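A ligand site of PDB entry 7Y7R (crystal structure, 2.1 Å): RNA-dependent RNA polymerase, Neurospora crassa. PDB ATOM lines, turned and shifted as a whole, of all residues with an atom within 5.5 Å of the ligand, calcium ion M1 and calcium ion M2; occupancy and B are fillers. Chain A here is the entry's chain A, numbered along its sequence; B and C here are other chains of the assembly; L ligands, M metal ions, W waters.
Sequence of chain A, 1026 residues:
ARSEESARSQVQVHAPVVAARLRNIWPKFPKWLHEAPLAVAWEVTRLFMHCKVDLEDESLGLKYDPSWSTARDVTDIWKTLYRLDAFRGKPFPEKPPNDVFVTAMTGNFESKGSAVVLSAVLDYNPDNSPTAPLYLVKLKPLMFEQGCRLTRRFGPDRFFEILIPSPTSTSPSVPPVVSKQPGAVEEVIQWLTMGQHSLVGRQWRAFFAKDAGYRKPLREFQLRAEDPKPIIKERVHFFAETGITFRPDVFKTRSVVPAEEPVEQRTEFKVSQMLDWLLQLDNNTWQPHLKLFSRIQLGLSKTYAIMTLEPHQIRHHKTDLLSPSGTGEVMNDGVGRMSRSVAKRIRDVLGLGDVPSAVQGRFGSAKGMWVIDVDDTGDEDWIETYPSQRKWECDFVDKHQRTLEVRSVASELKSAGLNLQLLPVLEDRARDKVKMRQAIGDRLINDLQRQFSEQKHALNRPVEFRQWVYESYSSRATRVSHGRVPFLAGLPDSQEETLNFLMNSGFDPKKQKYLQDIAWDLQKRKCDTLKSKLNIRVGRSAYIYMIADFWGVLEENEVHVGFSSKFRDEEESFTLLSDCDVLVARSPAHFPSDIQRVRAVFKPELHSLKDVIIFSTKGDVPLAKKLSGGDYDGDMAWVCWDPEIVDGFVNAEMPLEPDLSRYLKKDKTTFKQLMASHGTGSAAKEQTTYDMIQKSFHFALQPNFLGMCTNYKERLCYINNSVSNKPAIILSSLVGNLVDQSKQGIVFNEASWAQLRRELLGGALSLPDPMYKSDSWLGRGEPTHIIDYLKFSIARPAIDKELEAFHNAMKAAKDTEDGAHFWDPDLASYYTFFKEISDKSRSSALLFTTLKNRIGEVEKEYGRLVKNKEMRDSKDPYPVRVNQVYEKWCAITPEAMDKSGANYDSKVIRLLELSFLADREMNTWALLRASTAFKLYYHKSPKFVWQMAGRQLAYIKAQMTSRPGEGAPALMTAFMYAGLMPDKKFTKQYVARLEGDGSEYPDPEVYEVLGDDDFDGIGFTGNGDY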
ATOM      1  N   ARG A 295       5.273  16.397  -1.292  1.00  0.00           N
ATOM      2  CA  ARG A 295       5.463  17.824  -1.045  1.00  0.00           C
ATOM      3  C   ARG A 295       5.916  18.586  -2.293  1.00  0.00           C
ATOM      4  O   ARG A 295       5.955  19.822  -2.249  1.00  0.00           O
ATOM      5  CB  ARG A 295       6.469  18.047   0.076  1.00  0.00           C
ATOM      6  CG  ARG A 295       6.093  17.376   1.388  1.00  0.00           C
ATOM      7  CD  ARG A 295       4.629  17.578   1.705  1.00  0.00           C
ATOM      8  NE  ARG A 295       4.308  17.137   3.061  1.00  0.00           N
ATOM      9  CZ  ARG A 295       3.111  17.271   3.620  1.00  0.00           C
ATOM     10  NH1 ARG A 295       2.117  17.868   2.978  1.00  0.00           N
ATOM     11  NH2 ARG A 295       2.907  16.784   4.838  1.00  0.00           N
ATOM     12  N   ASP A 333      -2.983  23.742  14.359  1.00  0.00           N
ATOM     13  CA  ASP A 333      -2.433  22.983  13.253  1.00  0.00           C
ATOM     14  C   ASP A 333      -2.580  23.712  11.927  1.00  0.00           C
ATOM     15  O   ASP A 333      -3.705  23.845  11.421  1.00  0.00           O
ATOM     16  CB  ASP A 333      -3.135  21.616  13.220  1.00  0.00           C
ATOM     17  CG  ASP A 333      -2.508  20.631  12.241  1.00  0.00           C
ATOM     18  OD1 ASP A 333      -1.676  21.009  11.379  1.00  0.00           O
ATOM     19  OD2 ASP A 333      -2.902  19.445  12.333  1.00  0.00           O
ATOM     20  N   LYS A 367       3.102  25.654   4.821  1.00  0.00           N
ATOM     21  CA  LYS A 367       1.851  25.690   4.083  1.00  0.00           C
ATOM     22  C   LYS A 367       0.752  25.972   5.087  1.00  0.00           C
ATOM     23  O   LYS A 367       0.776  25.439   6.196  1.00  0.00           O
ATOM     24  CB  LYS A 367       1.605  24.332   3.341  1.00  0.00           C
ATOM     25  CG  LYS A 367       0.354  24.267   2.469  1.00  0.00           C
ATOM     26  CD  LYS A 367      -0.063  22.836   2.134  1.00  0.00           C
ATOM     27  CE  LYS A 367      -0.026  21.954   3.370  1.00  0.00           C
ATOM     28  NZ  LYS A 367      -1.341  21.849   4.116  1.00  0.00           N
ATOM     29  N   SER A 388       3.638  22.633  12.756  1.00  0.00           N
ATOM     30  CA  SER A 388       2.534  22.035  12.010  1.00  0.00           C
ATOM     31  C   SER A 388       2.470  22.583  10.590  1.00  0.00           C
ATOM     32  O   SER A 388       1.963  21.912   9.693  1.00  0.00           O
ATOM     33  CB  SER A 388       1.204  22.267  12.710  1.00  0.00           C
ATOM     34  OG  SER A 388       0.927  23.659  12.831  1.00  0.00           O
ATOM     35  N   LYS A 391       6.568  21.702   6.194  1.00  0.00           N
ATOM     36  CA  LYS A 391       6.434  20.335   5.718  1.00  0.00           C
ATOM     37  C   LYS A 391       7.771  19.689   5.415  1.00  0.00           C
ATOM     38  O   LYS A 391       7.821  18.492   5.120  1.00  0.00           O
ATOM     39  CB  LYS A 391       5.534  20.300   4.476  1.00  0.00           C
ATOM     40  CG  LYS A 391       4.107  20.758   4.700  1.00  0.00           C
ATOM     41  CD  LYS A 391       3.507  20.196   5.976  1.00  0.00           C
ATOM     42  CE  LYS A 391       2.023  20.557   6.089  1.00  0.00           C
ATOM     43  NZ  LYS A 391       1.492  20.258   7.454  1.00  0.00           N
ATOM     44  N   ARG A 586     -17.329  19.926   7.983  1.00  0.00           N
ATOM     45  CA  ARG A 586     -16.500  19.927   6.799  1.00  0.00           C
ATOM     46  C   ARG A 586     -17.023  18.871   5.831  1.00  0.00           C
ATOM     47  O   ARG A 586     -17.596  17.855   6.234  1.00  0.00           O
ATOM     48  CB  ARG A 586     -15.034  19.683   7.181  1.00  0.00           C
ATOM     49  CG  ARG A 586     -14.054  20.432   6.297  1.00  0.00           C
ATOM     50  CD  ARG A 586     -12.712  20.619   6.966  1.00  0.00           C
ATOM     51  NE  ARG A 586     -12.113  19.332   7.297  1.00  0.00           N
ATOM     52  CZ  ARG A 586     -11.407  18.578   6.461  1.00  0.00           C
ATOM     53  NH1 ARG A 586     -11.112  18.970   5.237  1.00  0.00           N
ATOM     54  NH2 ARG A 586     -10.994  17.384   6.881  1.00  0.00           N
ATOM     55  N   SER A 587     -16.859  19.139   4.548  1.00  0.00           N
ATOM     56  CA  SER A 587     -16.968  18.092   3.536  1.00  0.00           C
ATOM     57  C   SER A 587     -15.594  17.460   3.300  1.00  0.00           C
ATOM     58  O   SER A 587     -14.600  18.191   3.201  1.00  0.00           O
ATOM     59  CB  SER A 587     -17.487  18.665   2.238  1.00  0.00           C
ATOM     60  OG  SER A 587     -18.859  19.003   2.395  1.00  0.00           O
ATOM     61  N   PRO A 588     -15.484  16.123   3.236  1.00  0.00           N
ATOM     62  CA  PRO A 588     -16.568  15.135   3.294  1.00  0.00           C
ATOM     63  C   PRO A 588     -17.021  14.856   4.719  1.00  0.00           C
ATOM     64  O   PRO A 588     -16.164  14.702   5.591  1.00  0.00           O
ATOM     65  CB  PRO A 588     -15.925  13.882   2.687  1.00  0.00           C
ATOM     66  CG  PRO A 588     -14.478  13.974   3.096  1.00  0.00           C
ATOM     67  CD  PRO A 588     -14.153  15.468   3.182  1.00  0.00           C
ATOM     68  N   SER A 628     -14.152  15.856  10.528  1.00  0.00           N
ATOM     69  CA  SER A 628     -13.548  14.990   9.526  1.00  0.00           C
ATOM     70  C   SER A 628     -12.028  15.106   9.529  1.00  0.00           C
ATOM     71  O   SER A 628     -11.388  15.083   8.474  1.00  0.00           O
ATOM     72  CB  SER A 628     -14.136  15.302   8.139  1.00  0.00           C
ATOM     73  OG  SER A 628     -13.842  14.274   7.212  1.00  0.00           O
ATOM     74  N   GLY A 630     -10.108  17.717  10.326  1.00  0.00           N
ATOM     75  CA  GLY A 630      -9.662  18.960   9.714  1.00  0.00           C
ATOM     76  C   GLY A 630      -8.679  19.743  10.563  1.00  0.00           C
ATOM     77  O   GLY A 630      -8.224  19.300  11.619  1.00  0.00           O
ATOM     78  N   ASP A 631      -8.325  20.928  10.073  1.00  0.00           N
ATOM     79  CA  ASP A 631      -7.352  21.759  10.767  1.00  0.00           C
ATOM     80  C   ASP A 631      -7.436  23.175  10.196  1.00  0.00           C
ATOM     81  O   ASP A 631      -8.439  23.544   9.574  1.00  0.00           O
ATOM     82  CB  ASP A 631      -5.946  21.142  10.663  1.00  0.00           C
ATOM     83  CG  ASP A 631      -5.545  20.856   9.233  1.00  0.00           C
ATOM     84  OD1 ASP A 631      -6.074  21.494   8.303  1.00  0.00           O
ATOM     85  OD2 ASP A 631      -4.669  19.980   9.055  1.00  0.00           O
ATOM     86  N   ASP A 633      -5.296  24.866   7.960  1.00  0.00           N
ATOM     87  CA  ASP A 633      -4.330  25.137   6.883  1.00  0.00           C
ATOM     88  C   ASP A 633      -4.999  25.431   5.552  1.00  0.00           C
ATOM     89  O   ASP A 633      -4.356  25.314   4.509  1.00  0.00           O
ATOM     90  CB  ASP A 633      -3.352  23.974   6.742  1.00  0.00           C
ATOM     91  CG  ASP A 633      -4.003  22.713   6.209  1.00  0.00           C
ATOM     92  OD1 ASP A 633      -5.237  22.717   5.960  1.00  0.00           O
ATOM     93  OD2 ASP A 633      -3.282  21.703   6.048  1.00  0.00           O
ATOM     94  N   GLY A 634      -6.267  25.830   5.554  1.00  0.00           N
ATOM     95  CA  GLY A 634      -6.941  26.101   4.303  1.00  0.00           C
ATOM     96  C   GLY A 634      -8.299  25.433   4.273  1.00  0.00           C
ATOM     97  O   GLY A 634      -9.128  25.725   3.412  1.00  0.00           O
ATOM     98  N   ASP A 635      -8.517  24.522   5.224  1.00  0.00           N
ATOM     99  CA  ASP A 635      -9.833  23.932   5.429  1.00  0.00           C
ATOM    100  C   ASP A 635     -10.896  25.030   5.544  1.00  0.00           C
ATOM    101  O   ASP A 635     -10.659  26.070   6.174  1.00  0.00           O
ATOM    102  CB  ASP A 635      -9.840  23.087   6.723  1.00  0.00           C
ATOM    103  CG  ASP A 635      -9.054  21.756   6.591  1.00  0.00           C
ATOM    104  OD1 ASP A 635      -8.336  21.500   5.578  1.00  0.00           O
ATOM    105  OD2 ASP A 635      -9.149  20.950   7.536  1.00  0.00           O
ATOM    106  N   LEU A 706     -10.534   5.153  -3.317  1.00  0.00           N
ATOM    107  CA  LEU A 706     -11.359   6.160  -2.667  1.00  0.00           C
ATOM    108  C   LEU A 706     -12.765   6.174  -3.261  1.00  0.00           C
ATOM    109  O   LEU A 706     -13.755   6.149  -2.537  1.00  0.00           O
ATOM    110  CB  LEU A 706     -10.706   7.530  -2.799  1.00  0.00           C
ATOM    111  CG  LEU A 706     -11.490   8.644  -2.157  1.00  0.00           C
ATOM    112  CD1 LEU A 706     -11.820   8.302  -0.708  1.00  0.00           C
ATOM    113  CD2 LEU A 706     -10.700   9.911  -2.276  1.00  0.00           C
ATOM    114  N   VAL A 739      -8.287   8.982   1.705  1.00  0.00           N
ATOM    115  CA  VAL A 739      -8.025  10.314   1.149  1.00  0.00           C
ATOM    116  C   VAL A 739      -6.577  10.712   1.378  1.00  0.00           C
ATOM    117  O   VAL A 739      -5.990  11.415   0.558  1.00  0.00           O
ATOM    118  CB  VAL A 739      -8.970  11.408   1.685  1.00  0.00           C
ATOM    119  CG1 VAL A 739     -10.296  11.424   0.949  1.00  0.00           C
ATOM    120  CG2 VAL A 739      -9.184  11.277   3.182  1.00  0.00           C
ATOM    121  N   ASP A 740      -5.993  10.281   2.492  1.00  0.00           N
ATOM    122  CA  ASP A 740      -4.614  10.582   2.873  1.00  0.00           C
ATOM    123  C   ASP A 740      -3.594   9.690   2.162  1.00  0.00           C
ATOM    124  O   ASP A 740      -2.424   9.672   2.546  1.00  0.00           O
ATOM    125  CB  ASP A 740      -4.444  10.411   4.395  1.00  0.00           C
ATOM    126  CG  ASP A 740      -5.469  11.226   5.207  1.00  0.00           C
ATOM    127  OD1 ASP A 740      -6.273  11.963   4.604  1.00  0.00           O
ATOM    128  OD2 ASP A 740      -5.485  11.076   6.450  1.00  0.00           O
ATOM    129  N   LYS A 743      -0.044  10.796   0.316  1.00  0.00           N
ATOM    130  CA  LYS A 743       0.755  11.458   1.316  1.00  0.00           C
ATOM    131  C   LYS A 743       1.123  10.539   2.485  1.00  0.00           C
ATOM    132  O   LYS A 743       2.129  10.775   3.151  1.00  0.00           O
ATOM    133  CB  LYS A 743       0.018  12.699   1.837  1.00  0.00           C
ATOM    134  CG  LYS A 743       0.883  13.887   2.124  1.00  0.00           C
ATOM    135  CD  LYS A 743       0.063  15.102   2.564  1.00  0.00           C
ATOM    136  CE  LYS A 743      -0.643  15.763   1.395  1.00  0.00           C
ATOM    137  NZ  LYS A 743      -1.536  16.845   1.897  1.00  0.00           N
ATOM    138  P    DC B   7     -15.702   8.264  -8.748  1.00  0.00           P
ATOM    139  OP1  DC B   7     -16.950   8.268  -9.545  1.00  0.00           O
ATOM    140  OP2  DC B   7     -14.527   9.037  -9.200  1.00  0.00           O
ATOM    141  O5'  DC B   7     -16.029   8.745  -7.265  1.00  0.00           O
ATOM    142  C5'  DC B   7     -17.202   8.306  -6.603  1.00  0.00           C
ATOM    143  C4'  DC B   7     -17.375   9.081  -5.303  1.00  0.00           C
ATOM    144  O4'  DC B   7     -16.165   8.952  -4.522  1.00  0.00           O
ATOM    145  C3'  DC B   7     -17.563  10.579  -5.472  1.00  0.00           C
ATOM    146  O3'  DC B   7     -18.949  10.873  -5.664  1.00  0.00           O
ATOM    147  C2'  DC B   7     -17.051  11.127  -4.142  1.00  0.00           C
ATOM    148  C1'  DC B   7     -15.897  10.174  -3.843  1.00  0.00           C
ATOM    149  N1   DC B   7     -14.568  10.692  -4.314  1.00  0.00           N
ATOM    150  C2   DC B   7     -13.925  11.684  -3.561  1.00  0.00           C
ATOM    151  O2   DC B   7     -14.475  12.117  -2.528  1.00  0.00           O
ATOM    152  N3   DC B   7     -12.712  12.149  -3.976  1.00  0.00           N
ATOM    153  C4   DC B   7     -12.167  11.658  -5.092  1.00  0.00           C
ATOM    154  N4   DC B   7     -10.983  12.162  -5.473  1.00  0.00           N
ATOM    155  C5   DC B   7     -12.810  10.642  -5.881  1.00  0.00           C
ATOM    156  C6   DC B   7     -13.995  10.200  -5.446  1.00  0.00           C
ATOM    157  P    DC B   8     -19.383  12.281  -6.318  1.00  0.00           P
ATOM    158  OP1  DC B   8     -20.821  12.207  -6.653  1.00  0.00           O
ATOM    159  OP2  DC B   8     -18.389  12.624  -7.356  1.00  0.00           O
ATOM    160  O5'  DC B   8     -19.180  13.327  -5.128  1.00  0.00           O
ATOM    161  C5'  DC B   8     -19.970  13.229  -3.951  1.00  0.00           C
ATOM    162  C4'  DC B   8     -19.413  14.126  -2.854  1.00  0.00           C
ATOM    163  O4'  DC B   8     -18.058  13.743  -2.528  1.00  0.00           O
ATOM    164  C3'  DC B   8     -19.325  15.603  -3.200  1.00  0.00           C
ATOM    165  O3'  DC B   8     -20.553  16.174  -2.976  1.00  0.00           O
ATOM    166  C2'  DC B   8     -18.307  16.089  -2.197  1.00  0.00           C
ATOM    167  C1'  DC B   8     -17.356  14.900  -2.088  1.00  0.00           C
ATOM    168  N1   DC B   8     -16.074  15.066  -2.867  1.00  0.00           N
ATOM    169  C2   DC B   8     -15.025  15.746  -2.260  1.00  0.00           C
ATOM    170  O2   DC B   8     -15.184  16.184  -1.101  1.00  0.00           O
ATOM    171  N3   DC B   8     -13.855  15.891  -2.937  1.00  0.00           N
ATOM    172  C4   DC B   8     -13.728  15.397  -4.162  1.00  0.00           C
ATOM    173  N4   DC B   8     -12.550  15.571  -4.772  1.00  0.00           N
ATOM    174  C5   DC B   8     -14.790  14.684  -4.804  1.00  0.00           C
ATOM    175  C6   DC B   8     -15.947  14.557  -4.127  1.00  0.00           C
ATOM    176  P     G C   7      -4.499  22.453  -0.478  1.00  0.00           P
ATOM    177  OP1   G C   7      -3.547  22.846   0.594  1.00  0.00           O
ATOM    178  OP2   G C   7      -4.099  21.422  -1.480  1.00  0.00           O
ATOM    179  O5'   G C   7      -5.902  22.136   0.204  1.00  0.00           O
ATOM    180  C5'   G C   7      -6.403  22.956   1.270  1.00  0.00           C
ATOM    181  C4'   G C   7      -7.661  22.367   1.858  1.00  0.00           C
ATOM    182  O4'   G C   7      -8.697  22.304   0.848  1.00  0.00           O
ATOM    183  C3'   G C   7      -7.556  20.944   2.393  1.00  0.00           C
ATOM    184  C2'   G C   7      -9.006  20.448   2.332  1.00  0.00           C
ATOM    185  O2'   G C   7      -9.758  20.905   3.464  1.00  0.00           O
ATOM    186  C1'   G C   7      -9.511  21.168   1.070  1.00  0.00           C
ATOM    187  N9    G C   7      -9.481  20.329  -0.150  1.00  0.00           N
ATOM    188  C8    G C   7      -8.513  20.262  -1.106  1.00  0.00           C
ATOM    189  N7    G C   7      -8.808  19.441  -2.087  1.00  0.00           N
ATOM    190  C5    G C   7     -10.058  18.951  -1.731  1.00  0.00           C
ATOM    191  C6    G C   7     -10.892  18.014  -2.402  1.00  0.00           C
ATOM    192  O6    G C   7     -10.663  17.427  -3.459  1.00  0.00           O
ATOM    193  N1    G C   7     -12.083  17.807  -1.702  1.00  0.00           N
ATOM    194  C2    G C   7     -12.415  18.421  -0.524  1.00  0.00           C
ATOM    195  N2    G C   7     -13.598  18.098  -0.004  1.00  0.00           N
ATOM    196  N3    G C   7     -11.647  19.289   0.116  1.00  0.00           N
ATOM    197  C4    G C   7     -10.488  19.495  -0.546  1.00  0.00           C
HETATM  198  P1  LIG L   1      -0.741  17.979   5.466  1.00  0.00           P
HETATM  199  O1  LIG L   1      -0.609  18.343   4.000  1.00  0.00           O
HETATM  200  O2  LIG L   1       0.567  17.405   5.941  1.00  0.00           O
HETATM  201  O3  LIG L   1      -1.095  19.200   6.266  1.00  0.00           O
HETATM  202  O4  LIG L   1      -1.910  16.861   5.704  1.00  0.00           O
HETATM  203  P2  LIG L   1      -3.509  17.148   5.619  1.00  0.00           P
HETATM  204  O5  LIG L   1      -4.303  15.899   5.888  1.00  0.00           O
HETATM  205  O6  LIG L   1      -3.980  18.283   6.489  1.00  0.00           O
HETATM  206  O7  LIG L   1      -3.669  17.568   4.069  1.00  0.00           O
HETATM  207  P3  LIG L   1      -4.822  18.574   3.572  1.00  0.00           P
HETATM  208  O8  LIG L   1      -4.660  18.772   2.088  1.00  0.00           O
HETATM  209  O9  LIG L   1      -4.810  19.896   4.304  1.00  0.00           O
HETATM  210  O10 LIG L   1      -6.217  17.867   3.937  1.00  0.00           O
HETATM  211  C1  LIG L   1      -6.519  16.501   3.799  1.00  0.00           C
HETATM  212  C2  LIG L   1      -8.045  16.449   3.653  1.00  0.00           C
HETATM  213  O11 LIG L   1      -8.496  17.143   2.499  1.00  0.00           O
HETATM  214  C3  LIG L   1      -8.645  15.050   3.540  1.00  0.00           C
HETATM  215  C4  LIG L   1      -9.974  15.399   2.900  1.00  0.00           C
HETATM  216  O12 LIG L   1     -10.850  15.778   3.928  1.00  0.00           O
HETATM  217  C5  LIG L   1      -9.725  16.610   2.031  1.00  0.00           C
HETATM  218  N1  LIG L   1      -9.505  16.114   0.672  1.00  0.00           N
HETATM  219  C6  LIG L   1      -8.387  16.352  -0.091  1.00  0.00           C
HETATM  220  N2  LIG L   1      -8.535  15.708  -1.277  1.00  0.00           N
HETATM  221  C7  LIG L   1      -9.731  15.064  -1.284  1.00  0.00           C
HETATM  222  C8  LIG L   1     -10.386  14.268  -2.226  1.00  0.00           C
HETATM  223  O13 LIG L   1      -9.871  14.024  -3.318  1.00  0.00           O
HETATM  224  N3  LIG L   1     -11.613  13.744  -1.933  1.00  0.00           N
HETATM  225  C9  LIG L   1     -12.215  13.993  -0.728  1.00  0.00           C
HETATM  226  N4  LIG L   1     -13.404  13.475  -0.452  1.00  0.00           N
HETATM  227  N5  LIG L   1     -11.564  14.780   0.203  1.00  0.00           N
HETATM  228  C10 LIG L   1     -10.350  15.301  -0.057  1.00  0.00           C
HETATM  229 CA    CA M   1      -6.023  20.419   6.128  1.00  0.00          CA
HETATM  230 CA    CA M   2      -2.839  19.838   7.486  1.00  0.00          CA
HETATM  231 MG    MG M   3      -5.769  17.167   8.773  1.00  0.00          MG
HETATM  232  O   HOH W   1      -6.167  15.835  -2.782  1.00  0.00           O
HETATM  233  O   HOH W   2      -1.618  21.350   8.801  1.00  0.00           O
HETATM  234  O   HOH W   3      -8.757  16.412  -4.828  1.00  0.00           O
HETATM  235  O   HOH W   4      -5.342  18.851  -0.801  1.00  0.00           O
HETATM  236  O   HOH W   5      -2.597  18.279   9.296  1.00  0.00           O
HETATM  237  O   HOH W   6     -11.330  13.689   5.674  1.00  0.00           O
HETATM  238  O   HOH W   7      -7.259  18.710   6.973  1.00  0.00           O
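NH2 of Arg 295 lies within salt-bridge range of O2 of the ligand (2.7 Å).
O2 of DC 7 of chain B lies within hydrogen-bond range of a nitrogen (N4) of the ligand, 2.7 Å away.
NZ of Lys 743 lies within salt-bridge range of O1 of the ligand (2.7 Å).
The side-chain amino group (NZ) of Lys 391 is in salt-bridge range of an oxygen (O2) of the ligand (3.4 Å).
N3 of DC 8 of chain B sits at hydrogen-bond distance from a nitrogen (N3) of the ligand (3.3 Å).
NH2 of Arg 586 sits at hydrogen-bond distance from O12 of the ligand (3.4 Å).
NZ of Lys 367 lies within salt-bridge range of O1 of the ligand, 3.6 Å away.
OD2 of Asp 633 sits close to NZ of Lys 367 (2.7 Å).
O2' of G 7 of chain C sits close to the side-chain carboxylate (OD1) of Asp 635 (2.6 Å).
The side-chain carboxylate (OD2) of Asp 635 lies within salt-bridge range of the guanidinium group (NE) of Arg 586 (3.4 Å).
The side-chain amino group of Lys 391 sits at hydrogen-bond distance from the backbone carbonyl oxygen of Ser 388.
O2 of DC 8 of chain B sits close to N2 of G 7 of chain C.
O2' of G 7 of chain C sits at hydrogen-bond distance from NH1 of Arg 586, at 3.0 Å.
The guanidinium group (NH2) of Arg 586 is in hydrogen-bond range of the backbone carbonyl oxygen (O) of Ser 628 (2.8 Å).
The backbone carbonyl oxygen (O) of Pro 588 is in hydrogen-bond range of the side-chain hydroxyl (OG) of Ser 628, 2.9 Å away.
O6 of G 7 of chain C sits close to an oxygen (O13) of the ligand, 3.5 Å away.
CD of Pro 588 touches O12 of the ligand, at 3.4 Å.
Leu 706 touches the ligand (CD2 to N3, 3.96 Å).
Val 739 touches the ligand.
13 residues have an atom within 4 Å of the ligand: Arg 295, Lys 367, Lys 391, Arg 586, Pro 588, Asp 631, Asp 633, Leu 706, Val 739, Lys 743, DC 7 of chain B, DC 8 of chain B and G 7 of chain C.
Along chain A the residues within 4 Å of the ligand span positions 295 to 743.
Along chain A the residues within 4 Å of calcium ion M1 span positions 631 to 635.
The nearest printed residue that does not touch calcium ion M1 is G 7 of chain C (4.1 Å).
Of the 21 residues printed, 2 come within 4 Å of calcium ion M2.
Calcium ion M1 is bound by O9 of the ligand (2.3 Å).
Water W7 is bound to calcium ion M1 (2.3 Å).
The side-chain carboxylate (OD1) of Asp 631 binds calcium ion M1 (2.4 Å).
OD1 of Asp 633 binds calcium ion M1 (2.4 Å).
OD1 of Asp 635 binds calcium ion M1 (2.6 Å).
Slightly farther from calcium ion M1 lies an oxygen (O6) of the ligand (3.0 Å).
Slightly farther from calcium ion M1 lies OD2 of Asp 633 (3.0 Å).
Calcium ion M2 is bound by an oxygen (O6) of the ligand (2.2 Å), an oxygen (O3) of the ligand (2.2 Å), water W2 (2.3 Å), the side-chain carboxylate (OD2) of Asp 633 (2.4 Å), water W5 (2.4 Å) and the side-chain carboxylate (OD2) of Asp 631 (2.4 Å).
Water W7 bridges OD2 of Asp 635 and O10 of the ligand.
Water W6 lies within hydrogen-bond range of O12 of the ligand (2.8 Å) and OG of Ser 628 (3.0 Å).
Water W4 bridges OP2 of G 7 of chain C (2.9 Å) and an oxygen (O8) of the ligand (3.0 Å).
Water W3 lies within hydrogen-bond range of O6 of G 7 of chain C (2.6 Å) and an oxygen (O13) of the ligand (3.0 Å).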
